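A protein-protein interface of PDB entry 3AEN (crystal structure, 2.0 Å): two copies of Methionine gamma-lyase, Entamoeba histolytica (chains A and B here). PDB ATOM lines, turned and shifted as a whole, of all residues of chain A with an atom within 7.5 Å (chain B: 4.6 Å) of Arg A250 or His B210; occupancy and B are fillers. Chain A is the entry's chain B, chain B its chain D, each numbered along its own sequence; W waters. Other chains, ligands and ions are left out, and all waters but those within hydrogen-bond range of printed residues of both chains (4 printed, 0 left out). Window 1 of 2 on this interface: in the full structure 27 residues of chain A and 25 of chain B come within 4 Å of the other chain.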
ATOM      1  N   LEU A  11     -21.740  24.801  23.255  1.00  0.00           N
ATOM      2  CA  LEU A  11     -22.735  25.786  22.806  1.00  0.00           C
ATOM      3  C   LEU A  11     -23.107  25.650  21.335  1.00  0.00           C
ATOM      4  O   LEU A  11     -24.139  26.175  20.912  1.00  0.00           O
ATOM      5  CB  LEU A  11     -22.258  27.220  23.098  1.00  0.00           C
ATOM      6  CG  LEU A  11     -22.248  27.485  24.607  1.00  0.00           C
ATOM      7  CD1 LEU A  11     -21.560  28.794  24.946  1.00  0.00           C
ATOM      8  CD2 LEU A  11     -23.658  27.443  25.204  1.00  0.00           C
ATOM      9  N   HIS A  22     -34.000  27.365  17.186  1.00  0.00           N
ATOM     10  CA  HIS A  22     -32.676  27.658  17.795  1.00  0.00           C
ATOM     11  C   HIS A  22     -32.370  26.688  18.930  1.00  0.00           C
ATOM     12  O   HIS A  22     -31.298  26.073  18.965  1.00  0.00           O
ATOM     13  CB  HIS A  22     -32.602  29.108  18.284  1.00  0.00           C
ATOM     14  CG  HIS A  22     -31.303  29.472  18.950  1.00  0.00           C
ATOM     15  ND1 HIS A  22     -31.241  29.963  20.238  1.00  0.00           N
ATOM     16  CD2 HIS A  22     -30.027  29.454  18.496  1.00  0.00           C
ATOM     17  CE1 HIS A  22     -29.986  30.234  20.549  1.00  0.00           C
ATOM     18  NE2 HIS A  22     -29.225  29.929  19.511  1.00  0.00           N
ATOM     19  N   ALA A  23     -33.326  26.514  19.842  1.00  0.00           N
ATOM     20  CA  ALA A  23     -33.200  25.482  20.864  1.00  0.00           C
ATOM     21  C   ALA A  23     -33.627  24.157  20.250  1.00  0.00           C
ATOM     22  O   ALA A  23     -34.554  24.120  19.453  1.00  0.00           O
ATOM     23  CB  ALA A  23     -34.080  25.814  22.058  1.00  0.00           C
ATOM     24  N   GLN A  63     -28.908  14.164  20.898  1.00  0.00           N
ATOM     25  CA  GLN A  63     -28.225  15.455  20.909  1.00  0.00           C
ATOM     26  C   GLN A  63     -27.370  15.564  22.180  1.00  0.00           C
ATOM     27  O   GLN A  63     -26.200  15.965  22.114  1.00  0.00           O
ATOM     28  CB  GLN A  63     -29.209  16.658  20.775  1.00  0.00           C
ATOM     29  CG  GLN A  63     -28.471  17.975  20.355  1.00  0.00           C
ATOM     30  CD  GLN A  63     -28.793  19.205  21.244  1.00  0.00           C
ATOM     31  OE1 GLN A  63     -28.257  20.287  21.019  1.00  0.00           O
ATOM     32  NE2 GLN A  63     -29.671  19.032  22.250  1.00  0.00           N
ATOM     33  N   PHE A  64     -27.943  15.167  23.320  1.00  0.00           N
ATOM     34  CA  PHE A  64     -27.186  15.168  24.580  1.00  0.00           C
ATOM     35  C   PHE A  64     -26.030  14.158  24.533  1.00  0.00           C
ATOM     36  O   PHE A  64     -24.908  14.475  24.933  1.00  0.00           O
ATOM     37  CB  PHE A  64     -28.084  14.944  25.816  1.00  0.00           C
ATOM     38  CG  PHE A  64     -27.289  14.701  27.093  1.00  0.00           C
ATOM     39  CD1 PHE A  64     -27.182  13.426  27.634  1.00  0.00           C
ATOM     40  CD2 PHE A  64     -26.627  15.743  27.723  1.00  0.00           C
ATOM     41  CE1 PHE A  64     -26.440  13.200  28.782  1.00  0.00           C
ATOM     42  CE2 PHE A  64     -25.857  15.506  28.897  1.00  0.00           C
ATOM     43  CZ  PHE A  64     -25.775  14.244  29.409  1.00  0.00           C
ATOM     44  N   MET A  67     -23.100  15.620  22.593  1.00  0.00           N
ATOM     45  CA  MET A  67     -22.417  16.592  23.445  1.00  0.00           C
ATOM     46  C   MET A  67     -21.377  15.931  24.351  1.00  0.00           C
ATOM     47  O   MET A  67     -20.224  16.369  24.424  1.00  0.00           O
ATOM     48  CB  MET A  67     -23.438  17.332  24.315  1.00  0.00           C
ATOM     49  CG  MET A  67     -24.219  18.416  23.553  1.00  0.00           C
ATOM     50  SD  MET A  67     -25.447  19.267  24.575  1.00  0.00           S
ATOM     51  CE  MET A  67     -24.449  20.268  25.678  1.00  0.00           C
ATOM     52  N   ILE A 207     -22.678  17.311  35.614  1.00  0.00           N
ATOM     53  CA  ILE A 207     -22.928  17.507  34.172  1.00  0.00           C
ATOM     54  C   ILE A 207     -24.240  18.274  34.022  1.00  0.00           C
ATOM     55  O   ILE A 207     -24.266  19.371  33.422  1.00  0.00           O
ATOM     56  CB  ILE A 207     -22.836  16.174  33.330  1.00  0.00           C
ATOM     57  CG1 ILE A 207     -21.371  15.721  33.199  1.00  0.00           C
ATOM     58  CG2 ILE A 207     -23.396  16.357  31.915  1.00  0.00           C
ATOM     59  CD1 ILE A 207     -21.182  14.244  32.657  1.00  0.00           C
ATOM     60  N   ASN A 208     -25.309  17.742  34.621  1.00  0.00           N
ATOM     61  CA  ASN A 208     -26.553  18.514  34.702  1.00  0.00           C
ATOM     62  C   ASN A 208     -26.385  19.723  35.630  1.00  0.00           C
ATOM     63  O   ASN A 208     -26.779  20.845  35.283  1.00  0.00           O
ATOM     64  CB  ASN A 208     -27.722  17.683  35.189  1.00  0.00           C
ATOM     65  CG  ASN A 208     -29.020  18.475  35.150  1.00  0.00           C
ATOM     66  OD1 ASN A 208     -29.441  18.920  34.081  1.00  0.00           O
ATOM     67  ND2 ASN A 208     -29.631  18.704  36.316  1.00  0.00           N
ATOM     68  N   HIS A 210     -27.795  21.031  38.146  1.00  0.00           N
ATOM     69  CA  HIS A 210     -28.867  21.862  38.722  1.00  0.00           C
ATOM     70  C   HIS A 210     -29.789  21.111  39.721  1.00  0.00           C
ATOM     71  O   HIS A 210     -30.837  21.621  40.110  1.00  0.00           O
ATOM     72  CB  HIS A 210     -29.682  22.534  37.591  1.00  0.00           C
ATOM     73  CG  HIS A 210     -28.951  23.650  36.909  1.00  0.00           C
ATOM     74  ND1 HIS A 210     -27.892  23.433  36.051  1.00  0.00           N
ATOM     75  CD2 HIS A 210     -29.097  24.996  36.991  1.00  0.00           C
ATOM     76  CE1 HIS A 210     -27.428  24.597  35.620  1.00  0.00           C
ATOM     77  NE2 HIS A 210     -28.147  25.558  36.167  1.00  0.00           N
ATOM     78  N   ASP A 212     -31.928  18.692  39.449  1.00  0.00           N
ATOM     79  CA  ASP A 212     -33.331  18.498  39.092  1.00  0.00           C
ATOM     80  C   ASP A 212     -33.547  17.353  38.101  1.00  0.00           C
ATOM     81  O   ASP A 212     -34.633  17.214  37.532  1.00  0.00           O
ATOM     82  CB  ASP A 212     -33.942  19.827  38.590  1.00  0.00           C
ATOM     83  CG  ASP A 212     -33.108  20.488  37.483  1.00  0.00           C
ATOM     84  OD1 ASP A 212     -33.389  21.682  37.178  1.00  0.00           O
ATOM     85  OD2 ASP A 212     -32.200  19.816  36.899  1.00  0.00           O
ATOM     86  N   ASP A 244     -35.766  15.080  30.354  1.00  0.00           N
ATOM     87  CA  ASP A 244     -34.521  15.059  31.114  1.00  0.00           C
ATOM     88  C   ASP A 244     -33.292  15.324  30.218  1.00  0.00           C
ATOM     89  O   ASP A 244     -32.347  16.045  30.628  1.00  0.00           O
ATOM     90  CB  ASP A 244     -34.381  13.742  31.896  1.00  0.00           C
ATOM     91  CG  ASP A 244     -35.332  13.662  33.114  1.00  0.00           C
ATOM     92  OD1 ASP A 244     -35.366  12.622  33.782  1.00  0.00           O
ATOM     93  OD2 ASP A 244     -36.032  14.631  33.448  1.00  0.00           O
ATOM     94  N   ALA A 245     -33.300  14.772  29.005  1.00  0.00           N
ATOM     95  CA  ALA A 245     -32.197  15.038  28.043  1.00  0.00           C
ATOM     96  C   ALA A 245     -32.184  16.502  27.676  1.00  0.00           C
ATOM     97  O   ALA A 245     -31.112  17.094  27.537  1.00  0.00           O
ATOM     98  CB  ALA A 245     -32.323  14.174  26.762  1.00  0.00           C
ATOM     99  N   PHE A 246     -33.376  17.080  27.507  1.00  0.00           N
ATOM    100  CA  PHE A 246     -33.488  18.502  27.246  1.00  0.00           C
ATOM    101  C   PHE A 246     -32.860  19.273  28.412  1.00  0.00           C
ATOM    102  O   PHE A 246     -32.049  20.148  28.177  1.00  0.00           O
ATOM    103  CB  PHE A 246     -34.931  18.929  26.986  1.00  0.00           C
ATOM    104  CG  PHE A 246     -35.165  20.431  27.116  1.00  0.00           C
ATOM    105  CD1 PHE A 246     -35.026  21.270  26.009  1.00  0.00           C
ATOM    106  CD2 PHE A 246     -35.546  20.992  28.351  1.00  0.00           C
ATOM    107  CE1 PHE A 246     -35.257  22.655  26.107  1.00  0.00           C
ATOM    108  CE2 PHE A 246     -35.776  22.371  28.467  1.00  0.00           C
ATOM    109  CZ  PHE A 246     -35.630  23.197  27.329  1.00  0.00           C
ATOM    110  N   LEU A 247     -33.194  18.918  29.650  1.00  0.00           N
ATOM    111  CA  LEU A 247     -32.600  19.592  30.840  1.00  0.00           C
ATOM    112  C   LEU A 247     -31.105  19.354  31.044  1.00  0.00           C
ATOM    113  O   LEU A 247     -30.404  20.271  31.476  1.00  0.00           O
ATOM    114  CB  LEU A 247     -33.357  19.252  32.136  1.00  0.00           C
ATOM    115  CG  LEU A 247     -34.823  19.735  32.257  1.00  0.00           C
ATOM    116  CD1 LEU A 247     -35.509  19.064  33.471  1.00  0.00           C
ATOM    117  CD2 LEU A 247     -34.884  21.294  32.379  1.00  0.00           C
ATOM    118  N   CYS A 248     -30.615  18.142  30.759  1.00  0.00           N
ATOM    119  CA  CYS A 248     -29.170  17.834  30.903  1.00  0.00           C
ATOM    120  C   CYS A 248     -28.287  18.589  29.896  1.00  0.00           C
ATOM    121  O   CYS A 248     -27.214  19.117  30.264  1.00  0.00           O
ATOM    122  CB  CYS A 248     -28.913  16.319  30.791  1.00  0.00           C
ATOM    123  SG  CYS A 248     -29.582  15.425  32.191  1.00  0.00           S
ATOM    124  N   ALA A 249     -28.750  18.649  28.642  1.00  0.00           N
ATOM    125  CA  ALA A 249     -28.080  19.423  27.588  1.00  0.00           C
ATOM    126  C   ALA A 249     -28.030  20.888  27.972  1.00  0.00           C
ATOM    127  O   ALA A 249     -27.046  21.564  27.715  1.00  0.00           O
ATOM    128  CB  ALA A 249     -28.807  19.282  26.243  1.00  0.00           C
ATOM    129  N   ARG A 250     -29.131  21.376  28.538  1.00  0.00           N
ATOM    130  CA  ARG A 250     -29.250  22.773  28.918  1.00  0.00           C
ATOM    131  C   ARG A 250     -28.300  23.037  30.086  1.00  0.00           C
ATOM    132  O   ARG A 250     -27.623  24.057  30.103  1.00  0.00           O
ATOM    133  CB  ARG A 250     -30.693  23.082  29.310  1.00  0.00           C
ATOM    134  CG  ARG A 250     -30.995  24.552  29.554  1.00  0.00           C
ATOM    135  CD  ARG A 250     -32.288  24.620  30.339  1.00  0.00           C
ATOM    136  NE  ARG A 250     -33.063  25.844  30.127  1.00  0.00           N
ATOM    137  CZ  ARG A 250     -33.274  26.765  31.059  1.00  0.00           C
ATOM    138  NH1 ARG A 250     -34.049  27.793  30.783  1.00  0.00           N
ATOM    139  NH2 ARG A 250     -32.723  26.651  32.270  1.00  0.00           N
ATOM    140  N   GLY A 251     -28.247  22.107  31.049  1.00  0.00           N
ATOM    141  CA  GLY A 251     -27.343  22.227  32.194  1.00  0.00           C
ATOM    142  C   GLY A 251     -25.899  22.215  31.752  1.00  0.00           C
ATOM    143  O   GLY A 251     -25.062  22.950  32.279  1.00  0.00           O
ATOM    144  N   MET A 252     -25.613  21.391  30.758  1.00  0.00           N
ATOM    145  CA  MET A 252     -24.260  21.194  30.295  1.00  0.00           C
ATOM    146  C   MET A 252     -23.710  22.407  29.543  1.00  0.00           C
ATOM    147  O   MET A 252     -22.493  22.557  29.446  1.00  0.00           O
ATOM    148  CB  MET A 252     -24.180  19.944  29.426  1.00  0.00           C
ATOM    149  CG  MET A 252     -22.796  19.347  29.362  1.00  0.00           C
ATOM    150  SD  MET A 252     -22.770  17.864  28.367  1.00  0.00           S
ATOM    151  CE  MET A 252     -21.001  17.575  28.327  1.00  0.00           C
ATOM    152  N   LYS A 253     -24.595  23.260  29.004  1.00  0.00           N
ATOM    153  CA  LYS A 253     -24.162  24.535  28.380  1.00  0.00           C
ATOM    154  C   LYS A 253     -23.298  25.409  29.299  1.00  0.00           C
ATOM    155  O   LYS A 253     -22.466  26.197  28.806  1.00  0.00           O
ATOM    156  CB  LYS A 253     -25.354  25.387  27.892  1.00  0.00           C
ATOM    157  CG  LYS A 253     -26.333  24.740  26.888  1.00  0.00           C
ATOM    158  CD  LYS A 253     -25.621  23.987  25.769  1.00  0.00           C
ATOM    159  CE  LYS A 253     -26.515  23.718  24.557  1.00  0.00           C
ATOM    160  NZ  LYS A 253     -27.988  23.781  24.864  1.00  0.00           N
ATOM    161  N   THR A 254     -23.494  25.301  30.612  1.00  0.00           N
ATOM    162  CA  THR A 254     -22.691  26.083  31.568  1.00  0.00           C
ATOM    163  C   THR A 254     -21.672  25.242  32.330  1.00  0.00           C
ATOM    164  O   THR A 254     -21.064  25.723  33.289  1.00  0.00           O
ATOM    165  CB  THR A 254     -23.566  26.839  32.584  1.00  0.00           C
ATOM    166  OG1 THR A 254     -24.471  25.917  33.222  1.00  0.00           O
ATOM    167  CG2 THR A 254     -24.348  27.969  31.873  1.00  0.00           C
ATOM    168  N   LEU A 255     -21.460  24.004  31.891  1.00  0.00           N
ATOM    169  CA  LEU A 255     -20.593  23.095  32.617  1.00  0.00           C
ATOM    170  C   LEU A 255     -19.178  23.646  32.821  1.00  0.00           C
ATOM    171  O   LEU A 255     -18.679  23.620  33.954  1.00  0.00           O
ATOM    172  CB  LEU A 255     -20.554  21.702  31.969  1.00  0.00           C
ATOM    173  CG  LEU A 255     -19.677  20.657  32.684  1.00  0.00           C
ATOM    174  CD1 LEU A 255     -20.094  20.404  34.144  1.00  0.00           C
ATOM    175  CD2 LEU A 255     -19.612  19.333  31.907  1.00  0.00           C
ATOM    176  N   ARG A 258     -19.158  26.561  35.390  1.00  0.00           N
ATOM    177  CA  ARG A 258     -19.562  26.005  36.679  1.00  0.00           C
ATOM    178  C   ARG A 258     -18.423  25.204  37.308  1.00  0.00           C
ATOM    179  O   ARG A 258     -18.120  25.401  38.492  1.00  0.00           O
ATOM    180  CB  ARG A 258     -20.828  25.140  36.563  1.00  0.00           C
ATOM    181  CG  ARG A 258     -22.100  25.958  36.383  1.00  0.00           C
ATOM    182  CD  ARG A 258     -23.356  25.118  36.436  1.00  0.00           C
ATOM    183  NE  ARG A 258     -23.490  24.159  35.318  1.00  0.00           N
ATOM    184  CZ  ARG A 258     -23.200  22.850  35.358  1.00  0.00           C
ATOM    185  NH1 ARG A 258     -22.723  22.277  36.455  1.00  0.00           N
ATOM    186  NH2 ARG A 258     -23.396  22.098  34.287  1.00  0.00           N
ATOM    187  N   ASN B 208     -33.405  34.486  31.887  1.00  0.00           N
ATOM    188  CA  ASN B 208     -33.431  33.059  31.593  1.00  0.00           C
ATOM    189  C   ASN B 208     -32.137  32.603  30.909  1.00  0.00           C
ATOM    190  O   ASN B 208     -31.555  31.590  31.293  1.00  0.00           O
ATOM    191  CB  ASN B 208     -34.634  32.662  30.742  1.00  0.00           C
ATOM    192  CG  ASN B 208     -34.654  31.182  30.463  1.00  0.00           C
ATOM    193  OD1 ASN B 208     -34.827  30.370  31.381  1.00  0.00           O
ATOM    194  ND2 ASN B 208     -34.466  30.812  29.210  1.00  0.00           N
ATOM    195  N   GLY B 209     -31.722  33.352  29.886  1.00  0.00           N
ATOM    196  CA  GLY B 209     -30.397  33.211  29.288  1.00  0.00           C
ATOM    197  C   GLY B 209     -30.128  31.993  28.429  1.00  0.00           C
ATOM    198  O   GLY B 209     -29.030  31.892  27.869  1.00  0.00           O
ATOM    199  N   HIS B 210     -31.100  31.074  28.323  1.00  0.00           N
ATOM    200  CA  HIS B 210     -30.897  29.820  27.590  1.00  0.00           C
ATOM    201  C   HIS B 210     -31.700  29.657  26.281  1.00  0.00           C
ATOM    202  O   HIS B 210     -31.687  28.580  25.674  1.00  0.00           O
ATOM    203  CB  HIS B 210     -31.134  28.604  28.511  1.00  0.00           C
ATOM    204  CG  HIS B 210     -30.068  28.433  29.547  1.00  0.00           C
ATOM    205  ND1 HIS B 210     -29.967  29.260  30.642  1.00  0.00           N
ATOM    206  CD2 HIS B 210     -29.036  27.560  29.637  1.00  0.00           C
ATOM    207  CE1 HIS B 210     -28.921  28.900  31.370  1.00  0.00           C
ATOM    208  NE2 HIS B 210     -28.353  27.860  30.792  1.00  0.00           N
ATOM    209  N   GLY B 211     -32.365  30.725  25.853  1.00  0.00           N
ATOM    210  CA  GLY B 211     -33.050  30.754  24.575  1.00  0.00           C
ATOM    211  C   GLY B 211     -34.193  29.775  24.412  1.00  0.00           C
ATOM    212  O   GLY B 211     -34.527  29.396  23.283  1.00  0.00           O
ATOM    213  N   ASP B 212     -34.816  29.369  25.516  1.00  0.00           N
ATOM    214  CA  ASP B 212     -35.852  28.311  25.429  1.00  0.00           C
ATOM    215  C   ASP B 212     -37.146  28.678  26.130  1.00  0.00           C
ATOM    216  O   ASP B 212     -37.960  27.817  26.403  1.00  0.00           O
ATOM    217  CB  ASP B 212     -35.294  26.969  25.940  1.00  0.00           C
ATOM    218  CG  ASP B 212     -34.585  27.092  27.299  1.00  0.00           C
ATOM    219  OD1 ASP B 212     -33.892  26.116  27.696  1.00  0.00           O
ATOM    220  OD2 ASP B 212     -34.715  28.150  27.974  1.00  0.00           O
ATOM    221  N   VAL B 213     -37.303  29.954  26.459  1.00  0.00           N
ATOM    222  CA  VAL B 213     -38.458  30.478  27.187  1.00  0.00           C
ATOM    223  C   VAL B 213     -38.706  31.929  26.721  1.00  0.00           C
ATOM    224  O   VAL B 213     -37.762  32.696  26.512  1.00  0.00           O
ATOM    225  CB  VAL B 213     -38.237  30.511  28.732  1.00  0.00           C
ATOM    226  CG1 VAL B 213     -39.419  31.184  29.438  1.00  0.00           C
ATOM    227  CG2 VAL B 213     -38.002  29.116  29.321  1.00  0.00           C
ATOM    228  N   LEU B 247     -38.180  26.754  34.459  1.00  0.00           N
ATOM    229  CA  LEU B 247     -36.982  26.984  33.603  1.00  0.00           C
ATOM    230  C   LEU B 247     -36.323  28.344  33.829  1.00  0.00           C
ATOM    231  O   LEU B 247     -35.096  28.464  33.704  1.00  0.00           O
ATOM    232  CB  LEU B 247     -37.305  26.820  32.113  1.00  0.00           C
ATOM    233  CG  LEU B 247     -37.672  25.393  31.634  1.00  0.00           C
ATOM    234  CD1 LEU B 247     -38.211  25.453  30.180  1.00  0.00           C
ATOM    235  CD2 LEU B 247     -36.423  24.457  31.732  1.00  0.00           C
ATOM    236  N   ARG B 250     -34.382  28.295  37.123  1.00  0.00           N
ATOM    237  CA  ARG B 250     -33.218  27.452  36.860  1.00  0.00           C
ATOM    238  C   ARG B 250     -32.153  28.245  36.100  1.00  0.00           C
ATOM    239  O   ARG B 250     -30.991  28.248  36.500  1.00  0.00           O
ATOM    240  CB  ARG B 250     -33.638  26.227  36.041  1.00  0.00           C
ATOM    241  CG  ARG B 250     -32.558  25.208  35.878  1.00  0.00           C
ATOM    242  CD  ARG B 250     -32.931  24.233  34.802  1.00  0.00           C
ATOM    243  NE  ARG B 250     -32.430  22.879  35.041  1.00  0.00           N
ATOM    244  CZ  ARG B 250     -31.537  22.271  34.268  1.00  0.00           C
ATOM    245  NH1 ARG B 250     -31.205  21.034  34.511  1.00  0.00           N
ATOM    246  NH2 ARG B 250     -30.973  22.905  33.246  1.00  0.00           N
ATOM    247  N   GLY B 251     -32.547  28.933  35.028  1.00  0.00           N
ATOM    248  CA  GLY B 251     -31.606  29.763  34.266  1.00  0.00           C
ATOM    249  C   GLY B 251     -31.014  30.869  35.111  1.00  0.00           C
ATOM    250  O   GLY B 251     -29.834  31.207  35.004  1.00  0.00           O
ATOM    251  N   THR B 254     -27.558  30.681  37.282  1.00  0.00           N
ATOM    252  CA  THR B 254     -26.246  31.030  36.713  1.00  0.00           C
ATOM    253  C   THR B 254     -26.175  32.482  36.245  1.00  0.00           C
ATOM    254  O   THR B 254     -25.204  32.876  35.596  1.00  0.00           O
ATOM    255  CB  THR B 254     -25.828  30.091  35.560  1.00  0.00           C
ATOM    256  OG1 THR B 254     -26.858  30.075  34.567  1.00  0.00           O
ATOM    257  CG2 THR B 254     -25.587  28.635  36.091  1.00  0.00           C
ATOM    258  N   ARG B 258     -23.007  34.208  34.248  1.00  0.00           N
ATOM    259  CA  ARG B 258     -23.189  34.458  32.814  1.00  0.00           C
ATOM    260  C   ARG B 258     -22.998  35.945  32.484  1.00  0.00           C
ATOM    261  O   ARG B 258     -22.249  36.310  31.554  1.00  0.00           O
ATOM    262  CB  ARG B 258     -24.562  33.956  32.327  1.00  0.00           C
ATOM    263  CG  ARG B 258     -24.689  32.432  32.378  1.00  0.00           C
ATOM    264  CD  ARG B 258     -25.999  31.922  31.784  1.00  0.00           C
ATOM    265  NE  ARG B 258     -27.167  32.161  32.632  1.00  0.00           N
ATOM    266  CZ  ARG B 258     -28.037  33.169  32.484  1.00  0.00           C
ATOM    267  NH1 ARG B 258     -27.888  34.084  31.525  1.00  0.00           N
ATOM    268  NH2 ARG B 258     -29.064  33.271  33.311  1.00  0.00           N
ATOM    269  N   VAL B 336     -26.992  32.229  25.755  1.00  0.00           N
ATOM    270  CA  VAL B 336     -25.633  31.734  26.039  1.00  0.00           C
ATOM    271  C   VAL B 336     -24.735  31.676  24.787  1.00  0.00           C
ATOM    272  O   VAL B 336     -23.491  31.736  24.890  1.00  0.00           O
ATOM    273  CB  VAL B 336     -25.653  30.354  26.726  1.00  0.00           C
ATOM    274  CG1 VAL B 336     -26.022  30.483  28.224  1.00  0.00           C
ATOM    275  CG2 VAL B 336     -26.589  29.374  25.972  1.00  0.00           C
HETATM  276  O   HOH W   1     -28.817  27.978  34.980  1.00  0.00           O
HETATM  277  O   HOH W   2     -33.887  30.453  21.032  1.00  0.00           O
HETATM  278  O   HOH W   3     -30.074  25.966  33.103  1.00  0.00           O
HETATM  279  O   HOH W   4     -26.966  25.830  32.050  1.00  0.00           O
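Water W2 lies within hydrogen-bond range of O of Gly B211 (2.6 Å) and ND1 of His A22 (2.8 Å). Water W1 lies within hydrogen-bond range of O of Arg B250 (2.7 Å), NE2 of His A210 (2.8 Å), OG1 of Thr B254 (2.9 Å) and O of Gly B251 (3.4 Å). Water W4 lies within hydrogen-bond range of the backbone carbonyl oxygen of Arg A250 (2.7 Å), the side-chain hydroxyl of Thr A254 (2.8 Å), a ring nitrogen (NE2) of His B210 (2.8 Å) and the backbone carbonyl oxygen of Gly A251 (3.5 Å). Water W3 lies within hydrogen-bond range of NH2 of Arg A250 (2.9 Å), NH2 of Arg B250 (3.2 Å) and NE2 of His B210 (3.4 Å).
Leu A11 touches Val B336 (CD1 to O, 3.5 Å). Gly B211 touches Ala A23. His A210 touches Arg B250. Asp B212 touches Phe A246 (OD1 to CZ, 3.4 Å). Leu B247 touches Phe A246 (CD2 to CE2, 3.9 Å). CD2 of Leu B247 touches CD2 of Leu A247, at 3.6 Å. His B210 touches Arg A250 (CD2 to CG, 3.6 Å). Arg B250 touches Arg A250 (CD to NH2, 3.5 Å). Arg A250 touches Gly B251. Arg B250 touches Gly A251.
The side-chain amide nitrogen (ND2) of Asn B208 is in hydrogen-bond range of the side-chain carboxylate (OD2) of Asp B212. O of Gly B209 lies within hydrogen-bond range of N of Val B336. A ring nitrogen (ND1) of His B210 sits at hydrogen-bond distance from the backbone carbonyl oxygen of Asn B208 (2.9 Å). O of Asn A208 lies within hydrogen-bond range of ND1 of His A210 (2.9 Å). ND2 of Asn A208 is in hydrogen-bond range of OD2 of Asp A212 (2.9 Å). O of Gly A251 is in hydrogen-bond range of NH2 of Arg A258 (2.7 Å).
Asp A212 touches Arg B250, and with the chains exchanged Arg A250 touches Asp B212. Leu B247 touches its own counterpart, Leu A247. Leu A247 touches Arg B250, and with the chains exchanged Arg A250 touches Leu B247. Arg A250 touches its own counterpart, Arg B250. Positions printed for both chains: 208, 210, 212, 247, 250, 251, 254 and 258. Of the 16 pairs that touch across the chains among the printed residues, 12 have their exchanged pair printed and touching as well.
Of the printed residues of chain B, Asn A208 touches Arg B250. Printed residues of chain B within 4 Å of Asp A212: Arg B250 (2.6 Å). Of the printed residues of chain B, Phe A246 touches Asp B212 and Leu B247. No residue of chain A comes within 4 Å of Gly B209. Of chain A, only Arg A250 (3.6 Å) comes within 4 Å of His B210. Printed residues of chain A within 4 Å of Gly B211: Ala A23 (3.8 Å). Of the printed residues of chain A, Gly B251 touches Arg A250 (3.6 Å). The nearest residue of chain B that does not touch Arg A250 is Val B213 (4.4 Å). The nearest printed residue of chain B that does not touch Phe A246 is Arg B250 (5.9 Å).
Of the 23 printed residues of chain A, 9 touch a printed residue of chain B. Printed residues of chain A that touch a printed residue of chain B: Leu A11, Ala A23, Asn A208, His A210, Asp A212, Phe A246, Leu A247, Arg A250 and Gly A251. Hydrophobic or aromatic side chains of chain B that line the printed part of chain A: His B210, Leu B247 and Val B336. Among the printed residues, 16 pairs touch across the chains.
NH1 of Arg A250 lies within hydrogen-bond range of O of Leu B247 (3.2 Å). The side-chain amide oxygen (OD1) of Asn A208 lies within hydrogen-bond range of the guanidinium group (NH1) of Arg B250 (2.8 Å). NH1 of Arg A250 sits at hydrogen-bond distance from OD1 of Asn B208 (2.8 Å). NH2 of Arg B250 sits at hydrogen-bond distance from O of Leu A247 (3.2 Å). The guanidinium group (NE) of Arg B250 lies within salt-bridge range of the side-chain carboxylate (OD1) of Asp A212 (2.6 Å). OD1 of Asp B212 is in salt-bridge range of NE of Arg A250.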
